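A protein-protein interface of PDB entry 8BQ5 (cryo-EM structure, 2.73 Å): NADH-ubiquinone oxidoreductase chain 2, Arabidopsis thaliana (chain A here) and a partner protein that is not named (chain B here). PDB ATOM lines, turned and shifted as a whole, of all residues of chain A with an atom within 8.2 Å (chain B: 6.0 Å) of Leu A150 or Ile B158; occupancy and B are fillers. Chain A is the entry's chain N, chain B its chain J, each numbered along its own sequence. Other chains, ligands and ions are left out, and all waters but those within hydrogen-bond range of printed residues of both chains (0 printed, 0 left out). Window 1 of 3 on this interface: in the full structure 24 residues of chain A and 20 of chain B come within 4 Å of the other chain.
Leu A131 touches Val B161.
Asp A144 touches Trp B151.
Trp B151 touches Ile A146.
Trp B151 touches Ala A147 (NE1 to CB, 3.4 Å).
CD1 of Leu A150 touches O of Trp B151, at 3.7 Å.
O of Leu A150 touches CD1 of Ile B158, at 3.7 Å.
CB of Leu A154 touches CG1 of Ile B158, at 3.8 Å.
Leu A154 touches Val B161 (CD1 to CG2, 3.7 Å).
Leu A157 touches Ile B158.
CG2 of Val B161 touches SG of Cys A158, at 3.6 Å.
Along chain B the printed residues that touch a printed residue of chain A span positions 151 to 161.
Of the 24 printed residues of chain A, 8 touch a printed residue of chain B.
Printed residues of chain A that touch a printed residue of chain B: Leu A131, Asp A144, Ile A146, Ala A147, Leu A150, Leu A154, Leu A157 and Cys A158.
Hydrophobic or aromatic side chains of chain A that line the printed part of chain B: Leu A131, Ile A146, Ala A147, Leu A150, Leu A154 and Leu A157.
Among the printed residues, 10 pairs touch across the chains.
Among the printed residues, no Asp or Glu carboxylate lies within 4 Å of a Lys or Arg side-chain nitrogen of the other chain.
O of Leu A154 sits at hydrogen-bond distance from SG of Cys A158, 3.4 Å away.
The side-chain carboxylate of Asp A144 is in hydrogen-bond range of the backbone NH of Ile A146 (2.8 Å).
Of chain B, only Trp B151 (3.7 Å) and Ile B158 (3.7 Å) come within 4 Å of Leu A150.
Ile B158 touches just these residues of chain A: Leu A150, Leu A154 and Leu A157.
Of the printed residues of chain B, Leu A131 touches Val B161.
Of the printed residues of chain B, Asp A144 touches Trp B151 (3.9 Å).
Printed residues of chain A within 4 Å of Trp B151: Asp A144, Ile A146, Ala A147 and Leu A150.
Of the printed residues of chain B, Ile A146 touches Trp B151.
The nearest residue of chain B that does not touch Leu A150 is Val B154 (4.1 Å).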
ATOM      1  N   LEU A 131      15.682 -41.019   5.718  1.00  0.00           N
ATOM      2  CA  LEU A 131      15.462 -39.580   5.847  1.00  0.00           C
ATOM      3  C   LEU A 131      16.778 -38.821   5.992  1.00  0.00           C
ATOM      4  O   LEU A 131      16.935 -37.728   5.434  1.00  0.00           O
ATOM      5  CB  LEU A 131      14.529 -39.290   7.022  1.00  0.00           C
ATOM      6  CG  LEU A 131      13.091 -39.782   6.842  1.00  0.00           C
ATOM      7  CD1 LEU A 131      12.310 -39.680   8.139  1.00  0.00           C
ATOM      8  CD2 LEU A 131      12.399 -38.996   5.740  1.00  0.00           C
ATOM      9  N   GLY A 135      18.444 -35.954   3.648  1.00  0.00           N
ATOM     10  CA  GLY A 135      19.092 -34.758   4.162  1.00  0.00           C
ATOM     11  C   GLY A 135      20.486 -34.545   3.602  1.00  0.00           C
ATOM     12  O   GLY A 135      20.861 -33.424   3.260  1.00  0.00           O
ATOM     13  N   MET A 136      21.278 -35.614   3.506  1.00  0.00           N
ATOM     14  CA  MET A 136      22.630 -35.471   2.967  1.00  0.00           C
ATOM     15  C   MET A 136      22.605 -35.188   1.468  1.00  0.00           C
ATOM     16  O   MET A 136      23.448 -34.438   0.957  1.00  0.00           O
ATOM     17  CB  MET A 136      23.464 -36.713   3.275  1.00  0.00           C
ATOM     18  CG  MET A 136      23.848 -36.836   4.736  1.00  0.00           C
ATOM     19  SD  MET A 136      24.750 -38.347   5.105  1.00  0.00           S
ATOM     20  CE  MET A 136      23.460 -39.326   5.864  1.00  0.00           C
ATOM     21  N   PHE A 138      20.343 -33.373   0.064  1.00  0.00           N
ATOM     22  CA  PHE A 138      20.088 -31.939   0.010  1.00  0.00           C
ATOM     23  C   PHE A 138      21.301 -31.131   0.455  1.00  0.00           C
ATOM     24  O   PHE A 138      21.511 -30.016  -0.034  1.00  0.00           O
ATOM     25  CB  PHE A 138      18.867 -31.591   0.856  1.00  0.00           C
ATOM     26  CG  PHE A 138      17.566 -31.860   0.166  1.00  0.00           C
ATOM     27  CD1 PHE A 138      17.225 -31.174  -0.987  1.00  0.00           C
ATOM     28  CD2 PHE A 138      16.682 -32.800   0.667  1.00  0.00           C
ATOM     29  CE1 PHE A 138      16.029 -31.423  -1.627  1.00  0.00           C
ATOM     30  CE2 PHE A 138      15.484 -33.051   0.032  1.00  0.00           C
ATOM     31  CZ  PHE A 138      15.158 -32.362  -1.115  1.00  0.00           C
ATOM     32  N   MET A 139      22.101 -31.667   1.380  1.00  0.00           N
ATOM     33  CA  MET A 139      23.319 -30.976   1.790  1.00  0.00           C
ATOM     34  C   MET A 139      24.266 -30.808   0.612  1.00  0.00           C
ATOM     35  O   MET A 139      24.833 -29.729   0.405  1.00  0.00           O
ATOM     36  CB  MET A 139      24.031 -31.731   2.916  1.00  0.00           C
ATOM     37  CG  MET A 139      23.433 -31.541   4.295  1.00  0.00           C
ATOM     38  SD  MET A 139      24.077 -32.680   5.531  1.00  0.00           S
ATOM     39  CE  MET A 139      25.830 -32.379   5.348  1.00  0.00           C
ATOM     40  N   ALA A 142      23.176 -28.101  -1.695  1.00  0.00           N
ATOM     41  CA  ALA A 142      22.894 -26.809  -1.085  1.00  0.00           C
ATOM     42  C   ALA A 142      23.798 -25.729  -1.666  1.00  0.00           C
ATOM     43  O   ALA A 142      24.997 -25.936  -1.862  1.00  0.00           O
ATOM     44  CB  ALA A 142      23.074 -26.882   0.431  1.00  0.00           C
ATOM     45  N   ASP A 144      23.141 -22.223  -0.572  1.00  0.00           N
ATOM     46  CA  ASP A 144      22.745 -21.075   0.227  1.00  0.00           C
ATOM     47  C   ASP A 144      22.864 -21.479   1.688  1.00  0.00           C
ATOM     48  O   ASP A 144      22.702 -22.653   2.030  1.00  0.00           O
ATOM     49  CB  ASP A 144      21.318 -20.625  -0.121  1.00  0.00           C
ATOM     50  CG  ASP A 144      20.879 -19.380   0.636  1.00  0.00           C
ATOM     51  OD1 ASP A 144      20.969 -19.356   1.881  1.00  0.00           O
ATOM     52  OD2 ASP A 144      20.437 -18.415  -0.022  1.00  0.00           O
ATOM     53  N   LEU A 145      23.150 -20.497   2.545  1.00  0.00           N
ATOM     54  CA  LEU A 145      23.355 -20.794   3.961  1.00  0.00           C
ATOM     55  C   LEU A 145      22.096 -21.368   4.598  1.00  0.00           C
ATOM     56  O   LEU A 145      22.176 -22.257   5.454  1.00  0.00           O
ATOM     57  CB  LEU A 145      23.805 -19.537   4.704  1.00  0.00           C
ATOM     58  CG  LEU A 145      25.026 -18.816   4.135  1.00  0.00           C
ATOM     59  CD1 LEU A 145      24.992 -17.348   4.512  1.00  0.00           C
ATOM     60  CD2 LEU A 145      26.304 -19.469   4.627  1.00  0.00           C
ATOM     61  N   ILE A 146      20.925 -20.876   4.193  1.00  0.00           N
ATOM     62  CA  ILE A 146      19.670 -21.359   4.765  1.00  0.00           C
ATOM     63  C   ILE A 146      19.457 -22.831   4.424  1.00  0.00           C
ATOM     64  O   ILE A 146      19.193 -23.662   5.304  1.00  0.00           O
ATOM     65  CB  ILE A 146      18.499 -20.490   4.277  1.00  0.00           C
ATOM     66  CG1 ILE A 146      18.663 -19.053   4.777  1.00  0.00           C
ATOM     67  CG2 ILE A 146      17.176 -21.090   4.712  1.00  0.00           C
ATOM     68  CD1 ILE A 146      17.733 -18.055   4.125  1.00  0.00           C
ATOM     69  N   ALA A 147      19.577 -23.172   3.139  1.00  0.00           N
ATOM     70  CA  ALA A 147      19.406 -24.557   2.713  1.00  0.00           C
ATOM     71  C   ALA A 147      20.455 -25.460   3.346  1.00  0.00           C
ATOM     72  O   ALA A 147      20.146 -26.576   3.788  1.00  0.00           O
ATOM     73  CB  ALA A 147      19.475 -24.647   1.188  1.00  0.00           C
ATOM     74  N   MET A 148      21.701 -24.989   3.395  1.00  0.00           N
ATOM     75  CA  MET A 148      22.772 -25.758   4.016  1.00  0.00           C
ATOM     76  C   MET A 148      22.444 -26.073   5.469  1.00  0.00           C
ATOM     77  O   MET A 148      22.549 -27.226   5.907  1.00  0.00           O
ATOM     78  CB  MET A 148      24.087 -24.985   3.915  1.00  0.00           C
ATOM     79  CG  MET A 148      25.241 -25.614   4.668  1.00  0.00           C
ATOM     80  SD  MET A 148      26.749 -24.633   4.573  1.00  0.00           S
ATOM     81  CE  MET A 148      26.419 -23.378   5.809  1.00  0.00           C
ATOM     82  N   TYR A 149      22.023 -25.058   6.226  1.00  0.00           N
ATOM     83  CA  TYR A 149      21.703 -25.271   7.631  1.00  0.00           C
ATOM     84  C   TYR A 149      20.543 -26.240   7.796  1.00  0.00           C
ATOM     85  O   TYR A 149      20.593 -27.136   8.647  1.00  0.00           O
ATOM     86  CB  TYR A 149      21.380 -23.943   8.311  1.00  0.00           C
ATOM     87  CG  TYR A 149      20.920 -24.119   9.737  1.00  0.00           C
ATOM     88  CD1 TYR A 149      21.829 -24.407  10.743  1.00  0.00           C
ATOM     89  CD2 TYR A 149      19.579 -24.010  10.076  1.00  0.00           C
ATOM     90  CE1 TYR A 149      21.422 -24.574  12.044  1.00  0.00           C
ATOM     91  CE2 TYR A 149      19.160 -24.176  11.379  1.00  0.00           C
ATOM     92  CZ  TYR A 149      20.088 -24.457  12.358  1.00  0.00           C
ATOM     93  OH  TYR A 149      19.686 -24.624  13.661  1.00  0.00           O
ATOM     94  N   LEU A 150      19.484 -26.077   6.999  1.00  0.00           N
ATOM     95  CA  LEU A 150      18.308 -26.928   7.166  1.00  0.00           C
ATOM     96  C   LEU A 150      18.635 -28.388   6.866  1.00  0.00           C
ATOM     97  O   LEU A 150      18.207 -29.297   7.591  1.00  0.00           O
ATOM     98  CB  LEU A 150      17.166 -26.436   6.280  1.00  0.00           C
ATOM     99  CG  LEU A 150      16.525 -25.109   6.687  1.00  0.00           C
ATOM    100  CD1 LEU A 150      15.278 -24.857   5.867  1.00  0.00           C
ATOM    101  CD2 LEU A 150      16.202 -25.091   8.174  1.00  0.00           C
ATOM    102  N   ALA A 151      19.391 -28.632   5.794  1.00  0.00           N
ATOM    103  CA  ALA A 151      19.752 -30.004   5.453  1.00  0.00           C
ATOM    104  C   ALA A 151      20.680 -30.610   6.502  1.00  0.00           C
ATOM    105  O   ALA A 151      20.513 -31.778   6.895  1.00  0.00           O
ATOM    106  CB  ALA A 151      20.385 -30.038   4.065  1.00  0.00           C
ATOM    107  N   ILE A 152      21.649 -29.822   6.985  1.00  0.00           N
ATOM    108  CA  ILE A 152      22.523 -30.281   8.060  1.00  0.00           C
ATOM    109  C   ILE A 152      21.701 -30.673   9.280  1.00  0.00           C
ATOM    110  O   ILE A 152      21.980 -31.681   9.939  1.00  0.00           O
ATOM    111  CB  ILE A 152      23.559 -29.195   8.403  1.00  0.00           C
ATOM    112  CG1 ILE A 152      24.659 -29.133   7.342  1.00  0.00           C
ATOM    113  CG2 ILE A 152      24.159 -29.431   9.779  1.00  0.00           C
ATOM    114  CD1 ILE A 152      25.739 -28.120   7.656  1.00  0.00           C
ATOM    115  N   GLU A 153      20.669 -29.889   9.591  1.00  0.00           N
ATOM    116  CA  GLU A 153      19.895 -30.140  10.802  1.00  0.00           C
ATOM    117  C   GLU A 153      19.007 -31.370  10.657  1.00  0.00           C
ATOM    118  O   GLU A 153      18.836 -32.130  11.617  1.00  0.00           O
ATOM    119  CB  GLU A 153      19.064 -28.908  11.150  1.00  0.00           C
ATOM    120  CG  GLU A 153      19.890 -27.800  11.779  1.00  0.00           C
ATOM    121  CD  GLU A 153      20.300 -28.101  13.207  1.00  0.00           C
ATOM    122  OE1 GLU A 153      19.663 -27.581  14.140  1.00  0.00           O
ATOM    123  OE2 GLU A 153      21.260 -28.871  13.408  1.00  0.00           O
ATOM    124  N   LEU A 154      18.424 -31.581   9.475  1.00  0.00           N
ATOM    125  CA  LEU A 154      17.668 -32.812   9.247  1.00  0.00           C
ATOM    126  C   LEU A 154      18.566 -34.031   9.448  1.00  0.00           C
ATOM    127  O   LEU A 154      18.213 -34.984  10.168  1.00  0.00           O
ATOM    128  CB  LEU A 154      17.069 -32.794   7.839  1.00  0.00           C
ATOM    129  CG  LEU A 154      16.468 -34.070   7.248  1.00  0.00           C
ATOM    130  CD1 LEU A 154      15.335 -34.596   8.111  1.00  0.00           C
ATOM    131  CD2 LEU A 154      15.985 -33.817   5.830  1.00  0.00           C
ATOM    132  N   GLN A 155      19.758 -33.984   8.847  1.00  0.00           N
ATOM    133  CA  GLN A 155      20.750 -35.039   9.023  1.00  0.00           C
ATOM    134  C   GLN A 155      21.074 -35.272  10.501  1.00  0.00           C
ATOM    135  O   GLN A 155      21.042 -36.412  10.992  1.00  0.00           O
ATOM    136  CB  GLN A 155      21.999 -34.650   8.233  1.00  0.00           C
ATOM    137  CG  GLN A 155      23.063 -35.696   8.113  1.00  0.00           C
ATOM    138  CD  GLN A 155      24.418 -35.149   8.505  1.00  0.00           C
ATOM    139  OE1 GLN A 155      24.599 -34.650   9.614  1.00  0.00           O
ATOM    140  NE2 GLN A 155      25.375 -35.229   7.589  1.00  0.00           N
ATOM    141  N   SER A 156      21.371 -34.191  11.227  1.00  0.00           N
ATOM    142  CA  SER A 156      21.780 -34.311  12.622  1.00  0.00           C
ATOM    143  C   SER A 156      20.666 -34.873  13.494  1.00  0.00           C
ATOM    144  O   SER A 156      20.927 -35.669  14.400  1.00  0.00           O
ATOM    145  CB  SER A 156      22.235 -32.954  13.156  1.00  0.00           C
ATOM    146  OG  SER A 156      23.444 -32.546  12.544  1.00  0.00           O
ATOM    147  N   LEU A 157      19.424 -34.444  13.265  1.00  0.00           N
ATOM    148  CA  LEU A 157      18.322 -34.945  14.080  1.00  0.00           C
ATOM    149  C   LEU A 157      18.123 -36.439  13.866  1.00  0.00           C
ATOM    150  O   LEU A 157      17.921 -37.198  14.830  1.00  0.00           O
ATOM    151  CB  LEU A 157      17.046 -34.169  13.762  1.00  0.00           C
ATOM    152  CG  LEU A 157      17.059 -32.741  14.313  1.00  0.00           C
ATOM    153  CD1 LEU A 157      15.915 -31.930  13.746  1.00  0.00           C
ATOM    154  CD2 LEU A 157      17.021 -32.738  15.827  1.00  0.00           C
ATOM    155  N   CYS A 158      18.209 -36.889  12.609  1.00  0.00           N
ATOM    156  CA  CYS A 158      18.130 -38.325  12.359  1.00  0.00           C
ATOM    157  C   CYS A 158      19.244 -39.069  13.090  1.00  0.00           C
ATOM    158  O   CYS A 158      19.011 -40.125  13.697  1.00  0.00           O
ATOM    159  CB  CYS A 158      18.186 -38.604  10.858  1.00  0.00           C
ATOM    160  SG  CYS A 158      16.747 -38.032   9.932  1.00  0.00           S
ATOM    161  N   LEU A 190      27.403 -22.393  14.376  1.00  0.00           N
ATOM    162  CA  LEU A 190      27.370 -22.231  12.925  1.00  0.00           C
ATOM    163  C   LEU A 190      26.266 -21.273  12.490  1.00  0.00           C
ATOM    164  O   LEU A 190      26.459 -20.454  11.578  1.00  0.00           O
ATOM    165  CB  LEU A 190      27.194 -23.591  12.255  1.00  0.00           C
ATOM    166  CG  LEU A 190      27.071 -23.562  10.733  1.00  0.00           C
ATOM    167  CD1 LEU A 190      28.336 -23.024  10.104  1.00  0.00           C
ATOM    168  CD2 LEU A 190      26.765 -24.952  10.207  1.00  0.00           C
ATOM    169  N   LEU A 191      25.092 -21.369  13.118  1.00  0.00           N
ATOM    170  CA  LEU A 191      23.999 -20.466  12.779  1.00  0.00           C
ATOM    171  C   LEU A 191      24.361 -19.024  13.102  1.00  0.00           C
ATOM    172  O   LEU A 191      24.008 -18.102  12.356  1.00  0.00           O
ATOM    173  CB  LEU A 191      22.731 -20.880  13.519  1.00  0.00           C
ATOM    174  CG  LEU A 191      21.436 -20.519  12.799  1.00  0.00           C
ATOM    175  CD1 LEU A 191      21.515 -20.941  11.345  1.00  0.00           C
ATOM    176  CD2 LEU A 191      20.254 -21.162  13.492  1.00  0.00           C
ATOM    177  N   ASN A 276      29.915 -29.774   1.239  1.00  0.00           N
ATOM    178  CA  ASN A 276      29.523 -28.458   1.740  1.00  0.00           C
ATOM    179  C   ASN A 276      30.732 -27.551   1.944  1.00  0.00           C
ATOM    180  O   ASN A 276      30.716 -26.378   1.557  1.00  0.00           O
ATOM    181  CB  ASN A 276      28.759 -28.614   3.053  1.00  0.00           C
ATOM    182  CG  ASN A 276      27.279 -28.397   2.893  1.00  0.00           C
ATOM    183  OD1 ASN A 276      26.794 -28.119   1.798  1.00  0.00           O
ATOM    184  ND2 ASN A 276      26.545 -28.533   3.988  1.00  0.00           N
ATOM    185  N   TRP B 151      12.591 -25.183   1.055  1.00  0.00           N
ATOM    186  CA  TRP B 151      13.006 -25.065   2.452  1.00  0.00           C
ATOM    187  C   TRP B 151      11.835 -25.312   3.401  1.00  0.00           C
ATOM    188  O   TRP B 151      11.996 -25.931   4.460  1.00  0.00           O
ATOM    189  CB  TRP B 151      13.628 -23.687   2.691  1.00  0.00           C
ATOM    190  CG  TRP B 151      14.763 -23.347   1.751  1.00  0.00           C
ATOM    191  CD1 TRP B 151      15.472 -24.214   0.970  1.00  0.00           C
ATOM    192  CD2 TRP B 151      15.334 -22.052   1.525  1.00  0.00           C
ATOM    193  NE1 TRP B 151      16.435 -23.540   0.264  1.00  0.00           N
ATOM    194  CE2 TRP B 151      16.373 -22.211   0.588  1.00  0.00           C
ATOM    195  CE3 TRP B 151      15.061 -20.772   2.017  1.00  0.00           C
ATOM    196  CZ2 TRP B 151      17.141 -21.140   0.137  1.00  0.00           C
ATOM    197  CZ3 TRP B 151      15.827 -19.714   1.573  1.00  0.00           C
ATOM    198  CH2 TRP B 151      16.852 -19.902   0.638  1.00  0.00           C
ATOM    199  N   PHE B 152      10.647 -24.838   3.023  1.00  0.00           N
ATOM    200  CA  PHE B 152       9.414 -25.108   3.757  1.00  0.00           C
ATOM    201  C   PHE B 152       9.174 -26.613   3.907  1.00  0.00           C
ATOM    202  O   PHE B 152       8.933 -27.124   5.014  1.00  0.00           O
ATOM    203  CB  PHE B 152       8.277 -24.413   2.995  1.00  0.00           C
ATOM    204  CG  PHE B 152       6.905 -24.619   3.558  1.00  0.00           C
ATOM    205  CD1 PHE B 152       6.623 -24.345   4.883  1.00  0.00           C
ATOM    206  CD2 PHE B 152       5.872 -25.021   2.727  1.00  0.00           C
ATOM    207  CE1 PHE B 152       5.343 -24.514   5.376  1.00  0.00           C
ATOM    208  CE2 PHE B 152       4.597 -25.190   3.213  1.00  0.00           C
ATOM    209  CZ  PHE B 152       4.331 -24.935   4.538  1.00  0.00           C
ATOM    210  N   LEU B 153       9.284 -27.346   2.799  1.00  0.00           N
ATOM    211  CA  LEU B 153       9.048 -28.786   2.847  1.00  0.00           C
ATOM    212  C   LEU B 153      10.141 -29.514   3.630  1.00  0.00           C
ATOM    213  O   LEU B 153       9.866 -30.505   4.321  1.00  0.00           O
ATOM    214  CB  LEU B 153       8.925 -29.332   1.427  1.00  0.00           C
ATOM    215  CG  LEU B 153       7.741 -28.757   0.647  1.00  0.00           C
ATOM    216  CD1 LEU B 153       7.623 -29.401  -0.720  1.00  0.00           C
ATOM    217  CD2 LEU B 153       6.449 -28.923   1.434  1.00  0.00           C
ATOM    218  N   VAL B 154      11.386 -29.039   3.545  1.00  0.00           N
ATOM    219  CA  VAL B 154      12.453 -29.657   4.333  1.00  0.00           C
ATOM    220  C   VAL B 154      12.202 -29.451   5.823  1.00  0.00           C
ATOM    221  O   VAL B 154      12.474 -30.339   6.645  1.00  0.00           O
ATOM    222  CB  VAL B 154      13.830 -29.113   3.902  1.00  0.00           C
ATOM    223  CG1 VAL B 154      14.914 -29.606   4.847  1.00  0.00           C
ATOM    224  CG2 VAL B 154      14.143 -29.543   2.481  1.00  0.00           C
ATOM    225  N   SER B 155      11.672 -28.284   6.198  1.00  0.00           N
ATOM    226  CA  SER B 155      11.292 -28.066   7.591  1.00  0.00           C
ATOM    227  C   SER B 155      10.200 -29.041   8.022  1.00  0.00           C
ATOM    228  O   SER B 155      10.207 -29.544   9.157  1.00  0.00           O
ATOM    229  CB  SER B 155      10.839 -26.620   7.789  1.00  0.00           C
ATOM    230  OG  SER B 155       9.456 -26.480   7.516  1.00  0.00           O
ATOM    231  N   SER B 156       9.253 -29.325   7.125  1.00  0.00           N
ATOM    232  CA  SER B 156       8.260 -30.359   7.424  1.00  0.00           C
ATOM    233  C   SER B 156       8.919 -31.718   7.659  1.00  0.00           C
ATOM    234  O   SER B 156       8.511 -32.471   8.552  1.00  0.00           O
ATOM    235  CB  SER B 156       7.239 -30.461   6.295  1.00  0.00           C
ATOM    236  OG  SER B 156       7.718 -31.270   5.242  1.00  0.00           O
ATOM    237  N   LEU B 157       9.924 -32.056   6.849  1.00  0.00           N
ATOM    238  CA  LEU B 157      10.642 -33.316   7.051  1.00  0.00           C
ATOM    239  C   LEU B 157      11.309 -33.354   8.422  1.00  0.00           C
ATOM    240  O   LEU B 157      11.316 -34.393   9.100  1.00  0.00           O
ATOM    241  CB  LEU B 157      11.678 -33.513   5.946  1.00  0.00           C
ATOM    242  CG  LEU B 157      11.142 -33.976   4.593  1.00  0.00           C
ATOM    243  CD1 LEU B 157      12.291 -34.289   3.649  1.00  0.00           C
ATOM    244  CD2 LEU B 157      10.240 -35.185   4.774  1.00  0.00           C
ATOM    245  N   ILE B 158      11.875 -32.222   8.841  1.00  0.00           N
ATOM    246  CA  ILE B 158      12.474 -32.117  10.170  1.00  0.00           C
ATOM    247  C   ILE B 158      11.435 -32.406  11.253  1.00  0.00           C
ATOM    248  O   ILE B 158      11.688 -33.159  12.207  1.00  0.00           O
ATOM    249  CB  ILE B 158      13.115 -30.724  10.335  1.00  0.00           C
ATOM    250  CG1 ILE B 158      14.386 -30.618   9.487  1.00  0.00           C
ATOM    251  CG2 ILE B 158      13.402 -30.417  11.784  1.00  0.00           C
ATOM    252  CD1 ILE B 158      14.888 -29.201   9.301  1.00  0.00           C
ATOM    253  N   LEU B 159      10.239 -31.828  11.110  1.00  0.00           N
ATOM    254  CA  LEU B 159       9.190 -32.062  12.103  1.00  0.00           C
ATOM    255  C   LEU B 159       8.759 -33.528  12.134  1.00  0.00           C
ATOM    256  O   LEU B 159       8.499 -34.089  13.210  1.00  0.00           O
ATOM    257  CB  LEU B 159       7.995 -31.154  11.826  1.00  0.00           C
ATOM    258  CG  LEU B 159       8.267 -29.668  12.062  1.00  0.00           C
ATOM    259  CD1 LEU B 159       7.024 -28.849  11.777  1.00  0.00           C
ATOM    260  CD2 LEU B 159       8.765 -29.432  13.481  1.00  0.00           C
ATOM    261  N   LEU B 160       8.663 -34.160  10.962  1.00  0.00           N
ATOM    262  CA  LEU B 160       8.305 -35.576  10.916  1.00  0.00           C
ATOM    263  C   LEU B 160       9.341 -36.428  11.642  1.00  0.00           C
ATOM    264  O   LEU B 160       8.990 -37.374  12.367  1.00  0.00           O
ATOM    265  CB  LEU B 160       8.159 -36.033   9.465  1.00  0.00           C
ATOM    266  CG  LEU B 160       8.070 -37.543   9.243  1.00  0.00           C
ATOM    267  CD1 LEU B 160       6.771 -38.073   9.802  1.00  0.00           C
ATOM    268  CD2 LEU B 160       8.202 -37.894   7.769  1.00  0.00           C
ATOM    269  N   VAL B 161      10.625 -36.110  11.450  1.00  0.00           N
ATOM    270  CA  VAL B 161      11.676 -36.806  12.189  1.00  0.00           C
ATOM    271  C   VAL B 161      11.469 -36.633  13.687  1.00  0.00           C
ATOM    272  O   VAL B 161      11.636 -37.582  14.464  1.00  0.00           O
ATOM    273  CB  VAL B 161      13.066 -36.310  11.751  1.00  0.00           C
ATOM    274  CG1 VAL B 161      14.135 -36.823  12.701  1.00  0.00           C
ATOM    275  CG2 VAL B 161      13.364 -36.763  10.335  1.00  0.00           C
ATOM    276  N   ALA B 162      11.108 -35.422  14.116  1.00  0.00           N
ATOM    277  CA  ALA B 162      10.864 -35.193  15.540  1.00  0.00           C
ATOM    278  C   ALA B 162       9.763 -36.111  16.069  1.00  0.00           C
ATOM    279  O   ALA B 162       9.912 -36.731  17.129  1.00  0.00           O
ATOM    280  CB  ALA B 162      10.506 -33.727  15.788  1.00  0.00           C
ATOM    281  N   MET B 163       8.649 -36.212  15.336  1.00  0.00           N
ATOM    282  CA  MET B 163       7.545 -37.064  15.787  1.00  0.00           C
ATOM    283  C   MET B 163       7.976 -38.525  15.897  1.00  0.00           C
ATOM    284  O   MET B 163       7.740 -39.190  16.922  1.00  0.00           O
ATOM    285  CB  MET B 163       6.349 -36.935  14.840  1.00  0.00           C
ATOM    286  CG  MET B 163       6.075 -35.523  14.365  1.00  0.00           C
ATOM    287  SD  MET B 163       4.829 -35.418  13.064  1.00  0.00           S
ATOM    288  CE  MET B 163       3.370 -35.955  13.946  1.00  0.00           C
